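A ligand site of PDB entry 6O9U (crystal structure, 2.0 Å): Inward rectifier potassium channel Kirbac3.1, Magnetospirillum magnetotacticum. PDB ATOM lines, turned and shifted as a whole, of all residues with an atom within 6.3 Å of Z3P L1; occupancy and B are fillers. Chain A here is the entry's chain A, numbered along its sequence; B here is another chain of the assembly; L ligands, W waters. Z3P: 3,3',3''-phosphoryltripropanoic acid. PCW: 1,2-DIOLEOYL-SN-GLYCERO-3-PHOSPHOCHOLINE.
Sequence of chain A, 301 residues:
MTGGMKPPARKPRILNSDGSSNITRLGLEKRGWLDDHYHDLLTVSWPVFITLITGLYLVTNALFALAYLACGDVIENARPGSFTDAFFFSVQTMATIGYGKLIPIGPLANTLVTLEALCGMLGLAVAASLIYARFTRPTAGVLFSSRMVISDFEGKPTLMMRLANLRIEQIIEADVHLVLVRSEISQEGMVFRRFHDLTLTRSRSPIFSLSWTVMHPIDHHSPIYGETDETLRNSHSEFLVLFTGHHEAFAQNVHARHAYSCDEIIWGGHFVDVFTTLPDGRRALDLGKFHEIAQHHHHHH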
ATOM      1  N   ARG A 162      27.834  13.814  12.037  1.00  0.00           N
ATOM      2  CA  ARG A 162      26.810  14.851  12.024  1.00  0.00           C
ATOM      3  C   ARG A 162      25.420  14.265  12.275  1.00  0.00           C
ATOM      4  O   ARG A 162      25.198  13.058  12.163  1.00  0.00           O
ATOM      5  CB  ARG A 162      26.816  15.648  10.714  1.00  0.00           C
ATOM      6  CG  ARG A 162      26.711  14.871   9.415  1.00  0.00           C
ATOM      7  CD  ARG A 162      26.648  15.873   8.268  1.00  0.00           C
ATOM      8  NE  ARG A 162      26.601  15.258   6.947  1.00  0.00           N
ATOM      9  CZ  ARG A 162      26.782  15.916   5.809  1.00  0.00           C
ATOM     10  NH1 ARG A 162      27.023  17.223   5.825  1.00  0.00           N
ATOM     11  NH2 ARG A 162      26.729  15.277   4.647  1.00  0.00           N
ATOM     12  N   SER A 205      24.139  23.153  21.602  1.00  0.00           N
ATOM     13  CA  SER A 205      23.443  23.979  20.631  1.00  0.00           C
ATOM     14  C   SER A 205      22.182  24.518  21.283  1.00  0.00           C
ATOM     15  O   SER A 205      21.269  23.735  21.591  1.00  0.00           O
ATOM     16  CB  SER A 205      23.099  23.181  19.375  1.00  0.00           C
ATOM     17  OG  SER A 205      22.469  24.002  18.410  1.00  0.00           O
ATOM     18  N   ILE A 207      19.610  25.960  20.125  1.00  0.00           N
ATOM     19  CA  ILE A 207      18.464  25.508  19.334  1.00  0.00           C
ATOM     20  C   ILE A 207      18.994  24.645  18.199  1.00  0.00           C
ATOM     21  O   ILE A 207      19.572  25.170  17.233  1.00  0.00           O
ATOM     22  CB  ILE A 207      17.623  26.669  18.777  1.00  0.00           C
ATOM     23  CG1 ILE A 207      17.125  27.560  19.926  1.00  0.00           C
ATOM     24  CG2 ILE A 207      16.451  26.119  17.960  1.00  0.00           C
ATOM     25  CD1 ILE A 207      16.189  28.677  19.509  1.00  0.00           C
ATOM     26  N   PHE A 208      18.815  23.335  18.316  1.00  0.00           N
ATOM     27  CA  PHE A 208      19.095  22.424  17.219  1.00  0.00           C
ATOM     28  C   PHE A 208      17.886  22.414  16.284  1.00  0.00           C
ATOM     29  O   PHE A 208      16.763  22.104  16.706  1.00  0.00           O
ATOM     30  CB  PHE A 208      19.386  21.022  17.759  1.00  0.00           C
ATOM     31  CG  PHE A 208      19.506  19.966  16.696  1.00  0.00           C
ATOM     32  CD1 PHE A 208      20.586  19.961  15.831  1.00  0.00           C
ATOM     33  CD2 PHE A 208      18.554  18.971  16.585  1.00  0.00           C
ATOM     34  CE1 PHE A 208      20.706  18.986  14.851  1.00  0.00           C
ATOM     35  CE2 PHE A 208      18.667  17.987  15.613  1.00  0.00           C
ATOM     36  CZ  PHE A 208      19.740  18.002  14.752  1.00  0.00           C
ATOM     37  N   SER A 209      18.110  22.765  15.015  1.00  0.00           N
ATOM     38  CA  SER A 209      17.021  22.979  14.062  1.00  0.00           C
ATOM     39  C   SER A 209      17.044  21.960  12.923  1.00  0.00           C
ATOM     40  O   SER A 209      16.066  21.241  12.741  1.00  0.00           O
ATOM     41  CB  SER A 209      17.094  24.407  13.515  1.00  0.00           C
ATOM     42  OG  SER A 209      16.949  25.359  14.560  1.00  0.00           O
ATOM     43  N   LEU A 210      18.131  21.901  12.144  1.00  0.00           N
ATOM     44  CA  LEU A 210      18.157  21.108  10.928  1.00  0.00           C
ATOM     45  C   LEU A 210      19.299  20.100  10.896  1.00  0.00           C
ATOM     46  O   LEU A 210      19.045  18.893  10.767  1.00  0.00           O
ATOM     47  CB  LEU A 210      18.258  22.047   9.721  1.00  0.00           C
ATOM     48  CG  LEU A 210      17.082  23.016   9.570  1.00  0.00           C
ATOM     49  CD1 LEU A 210      17.399  24.080   8.528  1.00  0.00           C
ATOM     50  CD2 LEU A 210      15.811  22.269   9.213  1.00  0.00           C
ATOM     51  N   SER A 211      20.540  20.546  10.994  1.00  0.00           N
ATOM     52  CA  SER A 211      21.676  19.642  10.913  1.00  0.00           C
ATOM     53  C   SER A 211      22.832  20.237  11.716  1.00  0.00           C
ATOM     54  O   SER A 211      23.000  21.450  11.795  1.00  0.00           O
ATOM     55  CB  SER A 211      22.102  19.401   9.459  1.00  0.00           C
ATOM     56  OG  SER A 211      23.146  18.457   9.384  1.00  0.00           O
ATOM     57  N   TRP A 212      23.626  19.346  12.316  1.00  0.00           N
ATOM     58  CA  TRP A 212      24.683  19.739  13.236  1.00  0.00           C
ATOM     59  C   TRP A 212      25.875  18.808  13.034  1.00  0.00           C
ATOM     60  O   TRP A 212      25.742  17.598  13.200  1.00  0.00           O
ATOM     61  CB  TRP A 212      24.173  19.689  14.677  1.00  0.00           C
ATOM     62  CG  TRP A 212      25.132  20.165  15.730  1.00  0.00           C
ATOM     63  CD1 TRP A 212      26.342  20.769  15.535  1.00  0.00           C
ATOM     64  CD2 TRP A 212      24.952  20.088  17.147  1.00  0.00           C
ATOM     65  NE1 TRP A 212      26.927  21.063  16.748  1.00  0.00           N
ATOM     66  CE2 TRP A 212      26.082  20.652  17.759  1.00  0.00           C
ATOM     67  CE3 TRP A 212      23.924  19.580  17.957  1.00  0.00           C
ATOM     68  CZ2 TRP A 212      26.231  20.729  19.146  1.00  0.00           C
ATOM     69  CZ3 TRP A 212      24.071  19.662  19.336  1.00  0.00           C
ATOM     70  CH2 TRP A 212      25.213  20.225  19.906  1.00  0.00           C
ATOM     71  N   THR A 213      27.018  19.378  12.668  1.00  0.00           N
ATOM     72  CA  THR A 213      28.252  18.615  12.527  1.00  0.00           C
ATOM     73  C   THR A 213      29.021  18.693  13.829  1.00  0.00           C
ATOM     74  O   THR A 213      29.383  19.789  14.278  1.00  0.00           O
ATOM     75  CB  THR A 213      29.099  19.149  11.365  1.00  0.00           C
ATOM     76  OG1 THR A 213      28.347  19.075  10.150  1.00  0.00           O
ATOM     77  CG2 THR A 213      30.364  18.334  11.204  1.00  0.00           C
ATOM     78  N   VAL A 214      29.271  17.544  14.436  1.00  0.00           N
ATOM     79  CA  VAL A 214      29.915  17.439  15.737  1.00  0.00           C
ATOM     80  C   VAL A 214      31.392  17.155  15.505  1.00  0.00           C
ATOM     81  O   VAL A 214      31.743  16.259  14.739  1.00  0.00           O
ATOM     82  CB  VAL A 214      29.258  16.329  16.589  1.00  0.00           C
ATOM     83  CG1 VAL A 214      29.875  16.265  17.976  1.00  0.00           C
ATOM     84  CG2 VAL A 214      27.760  16.567  16.668  1.00  0.00           C
ATOM     85  N   VAL A 274      25.149  19.741   3.165  1.00  0.00           N
ATOM     86  CA  VAL A 274      23.716  19.559   3.014  1.00  0.00           C
ATOM     87  C   VAL A 274      22.971  20.889   2.906  1.00  0.00           C
ATOM     88  O   VAL A 274      21.814  20.907   2.444  1.00  0.00           O
ATOM     89  CB  VAL A 274      23.121  18.721   4.173  1.00  0.00           C
ATOM     90  CG1 VAL A 274      23.670  17.298   4.135  1.00  0.00           C
ATOM     91  CG2 VAL A 274      23.388  19.375   5.519  1.00  0.00           C
ATOM     92  N   PHE A 275      23.596  21.997   3.302  1.00  0.00           N
ATOM     93  CA  PHE A 275      23.014  23.323   3.114  1.00  0.00           C
ATOM     94  C   PHE A 275      23.479  23.891   1.793  1.00  0.00           C
ATOM     95  O   PHE A 275      24.659  23.783   1.433  1.00  0.00           O
ATOM     96  CB  PHE A 275      23.407  24.258   4.257  1.00  0.00           C
ATOM     97  CG  PHE A 275      22.795  23.887   5.579  1.00  0.00           C
ATOM     98  CD1 PHE A 275      21.538  24.346   5.934  1.00  0.00           C
ATOM     99  CD2 PHE A 275      23.490  23.095   6.474  1.00  0.00           C
ATOM    100  CE1 PHE A 275      20.978  24.016   7.148  1.00  0.00           C
ATOM    101  CE2 PHE A 275      22.932  22.760   7.697  1.00  0.00           C
ATOM    102  CZ  PHE A 275      21.675  23.223   8.029  1.00  0.00           C
ATOM    103  N   THR A 276      22.554  24.510   1.066  1.00  0.00           N
ATOM    104  CA  THR A 276      22.863  25.093  -0.232  1.00  0.00           C
ATOM    105  C   THR A 276      21.901  26.244  -0.504  1.00  0.00           C
ATOM    106  O   THR A 276      20.891  26.417   0.188  1.00  0.00           O
ATOM    107  CB  THR A 276      22.776  24.053  -1.347  1.00  0.00           C
ATOM    108  OG1 THR A 276      23.016  24.676  -2.613  1.00  0.00           O
ATOM    109  CG2 THR A 276      21.401  23.388  -1.357  1.00  0.00           C
ATOM    110  N   ARG A 283      17.794  29.658   0.574  1.00  0.00           N
ATOM    111  CA  ARG A 283      18.636  28.636   1.194  1.00  0.00           C
ATOM    112  C   ARG A 283      17.834  27.357   1.421  1.00  0.00           C
ATOM    113  O   ARG A 283      16.645  27.404   1.752  1.00  0.00           O
ATOM    114  CB  ARG A 283      19.198  29.158   2.513  1.00  0.00           C
ATOM    115  CG  ARG A 283      20.396  28.389   3.041  1.00  0.00           C
ATOM    116  CD  ARG A 283      21.374  29.328   3.732  1.00  0.00           C
ATOM    117  NE  ARG A 283      22.535  28.632   4.271  1.00  0.00           N
ATOM    118  CZ  ARG A 283      23.614  28.300   3.574  1.00  0.00           C
ATOM    119  NH1 ARG A 283      23.692  28.587   2.280  1.00  0.00           N
ATOM    120  NH2 ARG A 283      24.619  27.676   4.164  1.00  0.00           N
ATOM    121  N   ILE B  14      17.508  34.592   6.960  1.00  0.00           N
ATOM    122  CA  ILE B  14      17.331  33.152   7.172  1.00  0.00           C
ATOM    123  C   ILE B  14      16.433  32.902   8.374  1.00  0.00           C
ATOM    124  O   ILE B  14      15.404  32.229   8.276  1.00  0.00           O
ATOM    125  CB  ILE B  14      18.710  32.472   7.331  1.00  0.00           C
ATOM    126  CG1 ILE B  14      19.553  32.702   6.078  1.00  0.00           C
ATOM    127  CG2 ILE B  14      18.530  30.977   7.593  1.00  0.00           C
ATOM    128  CD1 ILE B  14      21.002  32.265   6.220  1.00  0.00           C
ATOM    129  N   ILE B  23      14.751  28.296   5.693  1.00  0.00           N
ATOM    130  CA  ILE B  23      15.473  27.323   4.884  1.00  0.00           C
ATOM    131  C   ILE B  23      14.481  26.327   4.306  1.00  0.00           C
ATOM    132  O   ILE B  23      13.649  25.756   5.023  1.00  0.00           O
ATOM    133  CB  ILE B  23      16.551  26.626   5.731  1.00  0.00           C
ATOM    134  CG1 ILE B  23      17.574  27.663   6.206  1.00  0.00           C
ATOM    135  CG2 ILE B  23      17.255  25.532   4.914  1.00  0.00           C
ATOM    136  CD1 ILE B  23      18.593  27.143   7.206  1.00  0.00           C
ATOM    137  N   VAL B 181      25.038  33.898  14.342  1.00  0.00           N
ATOM    138  CA  VAL B 181      25.090  32.969  13.223  1.00  0.00           C
ATOM    139  C   VAL B 181      25.623  33.748  12.024  1.00  0.00           C
ATOM    140  O   VAL B 181      25.056  34.787  11.665  1.00  0.00           O
ATOM    141  CB  VAL B 181      23.726  32.355  12.908  1.00  0.00           C
ATOM    142  CG1 VAL B 181      23.848  31.296  11.817  1.00  0.00           C
ATOM    143  CG2 VAL B 181      23.097  31.747  14.165  1.00  0.00           C
ATOM    144  N   PHE B 192      31.411  28.063   5.299  1.00  0.00           N
ATOM    145  CA  PHE B 192      30.389  27.422   6.111  1.00  0.00           C
ATOM    146  C   PHE B 192      29.731  28.475   7.001  1.00  0.00           C
ATOM    147  O   PHE B 192      30.302  29.540   7.240  1.00  0.00           O
ATOM    148  CB  PHE B 192      31.001  26.313   6.975  1.00  0.00           C
ATOM    149  CG  PHE B 192      32.104  26.783   7.889  1.00  0.00           C
ATOM    150  CD1 PHE B 192      33.409  26.865   7.422  1.00  0.00           C
ATOM    151  CD2 PHE B 192      31.837  27.152   9.196  1.00  0.00           C
ATOM    152  CE1 PHE B 192      34.419  27.304   8.247  1.00  0.00           C
ATOM    153  CE2 PHE B 192      32.848  27.591  10.022  1.00  0.00           C
ATOM    154  CZ  PHE B 192      34.143  27.669   9.554  1.00  0.00           C
ATOM    155  N   ARG B 193      28.537  28.153   7.469  1.00  0.00           N
ATOM    156  CA  ARG B 193      27.875  28.916   8.515  1.00  0.00           C
ATOM    157  C   ARG B 193      27.982  28.160   9.828  1.00  0.00           C
ATOM    158  O   ARG B 193      27.801  26.946   9.877  1.00  0.00           O
ATOM    159  CB  ARG B 193      26.408  29.187   8.170  1.00  0.00           C
ATOM    160  CG  ARG B 193      26.201  30.362   7.220  1.00  0.00           C
ATOM    161  CD  ARG B 193      24.733  30.552   6.843  1.00  0.00           C
ATOM    162  NE  ARG B 193      23.977  31.313   7.847  1.00  0.00           N
ATOM    163  CZ  ARG B 193      24.144  32.604   8.095  1.00  0.00           C
ATOM    164  NH1 ARG B 193      25.052  33.310   7.431  1.00  0.00           N
ATOM    165  NH2 ARG B 193      23.406  33.208   9.018  1.00  0.00           N
ATOM    166  N   ARG B 194      28.290  28.894  10.896  1.00  0.00           N
ATOM    167  CA  ARG B 194      28.371  28.323  12.235  1.00  0.00           C
ATOM    168  C   ARG B 194      27.759  29.301  13.222  1.00  0.00           C
ATOM    169  O   ARG B 194      27.461  30.449  12.876  1.00  0.00           O
ATOM    170  CB  ARG B 194      29.815  27.996  12.620  1.00  0.00           C
ATOM    171  CG  ARG B 194      30.752  29.181  12.607  1.00  0.00           C
ATOM    172  CD  ARG B 194      31.622  29.220  13.857  1.00  0.00           C
ATOM    173  NE  ARG B 194      32.281  27.940  14.109  1.00  0.00           N
ATOM    174  CZ  ARG B 194      33.532  27.639  13.756  1.00  0.00           C
ATOM    175  NH1 ARG B 194      34.289  28.521  13.117  1.00  0.00           N
ATOM    176  NH2 ARG B 194      34.028  26.450  14.050  1.00  0.00           N
ATOM    177  N   PHE B 195      27.584  28.849  14.457  1.00  0.00           N
ATOM    178  CA  PHE B 195      27.030  29.697  15.500  1.00  0.00           C
ATOM    179  C   PHE B 195      28.051  29.914  16.604  1.00  0.00           C
ATOM    180  O   PHE B 195      28.932  29.072  16.854  1.00  0.00           O
ATOM    181  CB  PHE B 195      25.724  29.092  16.081  1.00  0.00           C
ATOM    182  CG  PHE B 195      25.904  27.778  16.774  1.00  0.00           C
ATOM    183  CD1 PHE B 195      26.230  27.723  18.125  1.00  0.00           C
ATOM    184  CD2 PHE B 195      25.726  26.578  16.093  1.00  0.00           C
ATOM    185  CE1 PHE B 195      26.376  26.504  18.769  1.00  0.00           C
ATOM    186  CE2 PHE B 195      25.870  25.364  16.729  1.00  0.00           C
ATOM    187  CZ  PHE B 195      26.204  25.319  18.072  1.00  0.00           C
HETATM  188  O01 Z3P L   1      20.816  23.320  14.176  1.00  0.00           O
HETATM  189  C02 Z3P L   1      21.120  23.790  13.048  1.00  0.00           C
HETATM  190  O03 Z3P L   1      20.360  23.609  12.059  1.00  0.00           O
HETATM  191  C04 Z3P L   1      22.417  24.565  12.868  1.00  0.00           C
HETATM  192  C05 Z3P L   1      22.710  24.827  11.393  1.00  0.00           C
HETATM  193  P06 Z3P L   1      24.287  25.772  11.155  1.00  0.00           P
HETATM  194  O07 Z3P L   1      24.361  27.013  11.966  1.00  0.00           O
HETATM  195  C08 Z3P L   1      24.389  26.087   9.324  1.00  0.00           C
HETATM  196  C09 Z3P L   1      23.154  26.812   8.799  1.00  0.00           C
HETATM  197  C10 Z3P L   1      23.230  27.113   7.304  1.00  0.00           C
HETATM  198  O11 Z3P L   1      24.239  26.769   6.639  1.00  0.00           O
HETATM  199  O12 Z3P L   1      22.285  27.719   6.749  1.00  0.00           O
HETATM  200  C13 Z3P L   1      25.674  24.590  11.554  1.00  0.00           C
HETATM  201  C14 Z3P L   1      25.573  23.305  10.717  1.00  0.00           C
HETATM  202  C15 Z3P L   1      26.605  22.248  11.090  1.00  0.00           C
HETATM  203  O16 Z3P L   1      27.146  22.263  12.227  1.00  0.00           O
HETATM  204  O17 Z3P L   1      26.904  21.354  10.263  1.00  0.00           O
HETATM  205  C4  PCW L   2      30.707  23.613   9.081  1.00  0.00           C
HETATM  206  C5  PCW L   2      30.633  22.743  10.331  1.00  0.00           C
HETATM  207  C6  PCW L   2      29.632  24.631  11.338  1.00  0.00           C
HETATM  208  C7  PCW L   2      31.922  24.150  11.723  1.00  0.00           C
HETATM  209  C8  PCW L   2      30.246  22.762  12.658  1.00  0.00           C
HETATM  210  N   PCW L   2      30.604  23.576  11.513  1.00  0.00           N
HETATM  211  O1P PCW L   2      32.817  21.006   9.312  1.00  0.00           O
HETATM  212  O2P PCW L   2      33.537  21.990   7.037  1.00  0.00           O
HETATM  213  O3P PCW L   2      31.192  21.273   7.322  1.00  0.00           O
HETATM  214  O4P PCW L   2      31.974  23.429   8.508  1.00  0.00           O
HETATM  215  P   PCW L   2      32.379  21.907   8.008  1.00  0.00           P
HETATM  216  O   HOH W   1      22.637  23.026  16.012  1.00  0.00           O
HETATM  217  O   HOH W   2      25.404  19.784   8.655  1.00  0.00           O
HETATM  218  O   HOH W   3      21.982  29.782   8.755  1.00  0.00           O
HETATM  219  O   HOH W   4      26.555  25.741   6.450  1.00  0.00           O
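Water W4 lies within hydrogen-bond range of an oxygen (O11) of Z3P L1 (2.5 Å) and the backbone NH (N) of Arg 193 of chain B (3.3 Å).
Water W1 bridges the side-chain hydroxyl (OG) of Ser 205 and an oxygen (O01) of Z3P L1.
Water W2 lies within hydrogen-bond range of an oxygen (O17) of Z3P L1 (2.7 Å), the side-chain hydroxyl (OG) of Ser 211 (2.7 Å) and the side-chain hydroxyl (OG1) of Thr 213 (3.4 Å).
Water W3 lies within hydrogen-bond range of NE of Arg 193 of chain B (2.7 Å) and O12 of Z3P L1 (2.9 Å).
Ile 207 touches Z3P L1.
CA of Phe 208 touches O01 of Z3P L1 (3.6 Å).
Trp 212 touches Z3P L1 (CA to O16, 3.7 Å).
CG of Phe 275 touches O11 of Z3P L1, 3.4 Å away.
CD1 of Ile 23 of chain B touches O12 of Z3P L1, 3.8 Å away.
Arg 193 of chain B touches Z3P L1 (O to C08, 3.6 Å).
Within 4 Å of Z3P L1: Ile 207, Phe 208, Ser 209, Leu 210, Ser 211, Trp 212, Thr 213, Phe 275, Arg 283, Ile 23 of chain B and Arg 193 of chain B.
The nearest printed residue that does not touch Z3P L1 is Arg 194 of chain B (4.2 Å).
O12 of Z3P L1 is in salt-bridge range of NE of Arg 283, at 2.7 Å.
N of Thr 213 lies within hydrogen-bond range of O16 of Z3P L1 (2.9 Å).
The side-chain hydroxyl of Thr 213 lies within hydrogen-bond range of an oxygen (O17) of Z3P L1.
An oxygen (O03) of Z3P L1 lies within hydrogen-bond range of the backbone NH (N) of Leu 210 (2.8 Å).
An oxygen (O01) of Z3P L1 is in hydrogen-bond range of the backbone NH of Ser 209, at 2.9 Å.
The backbone NH (N) of Ser 211 is in hydrogen-bond range of an oxygen (O03) of Z3P L1.
The backbone carbonyl oxygen (O) of Ile 207 lies within hydrogen-bond range of the side-chain hydroxyl (OG) of Ser 205, 3.3 Å away.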
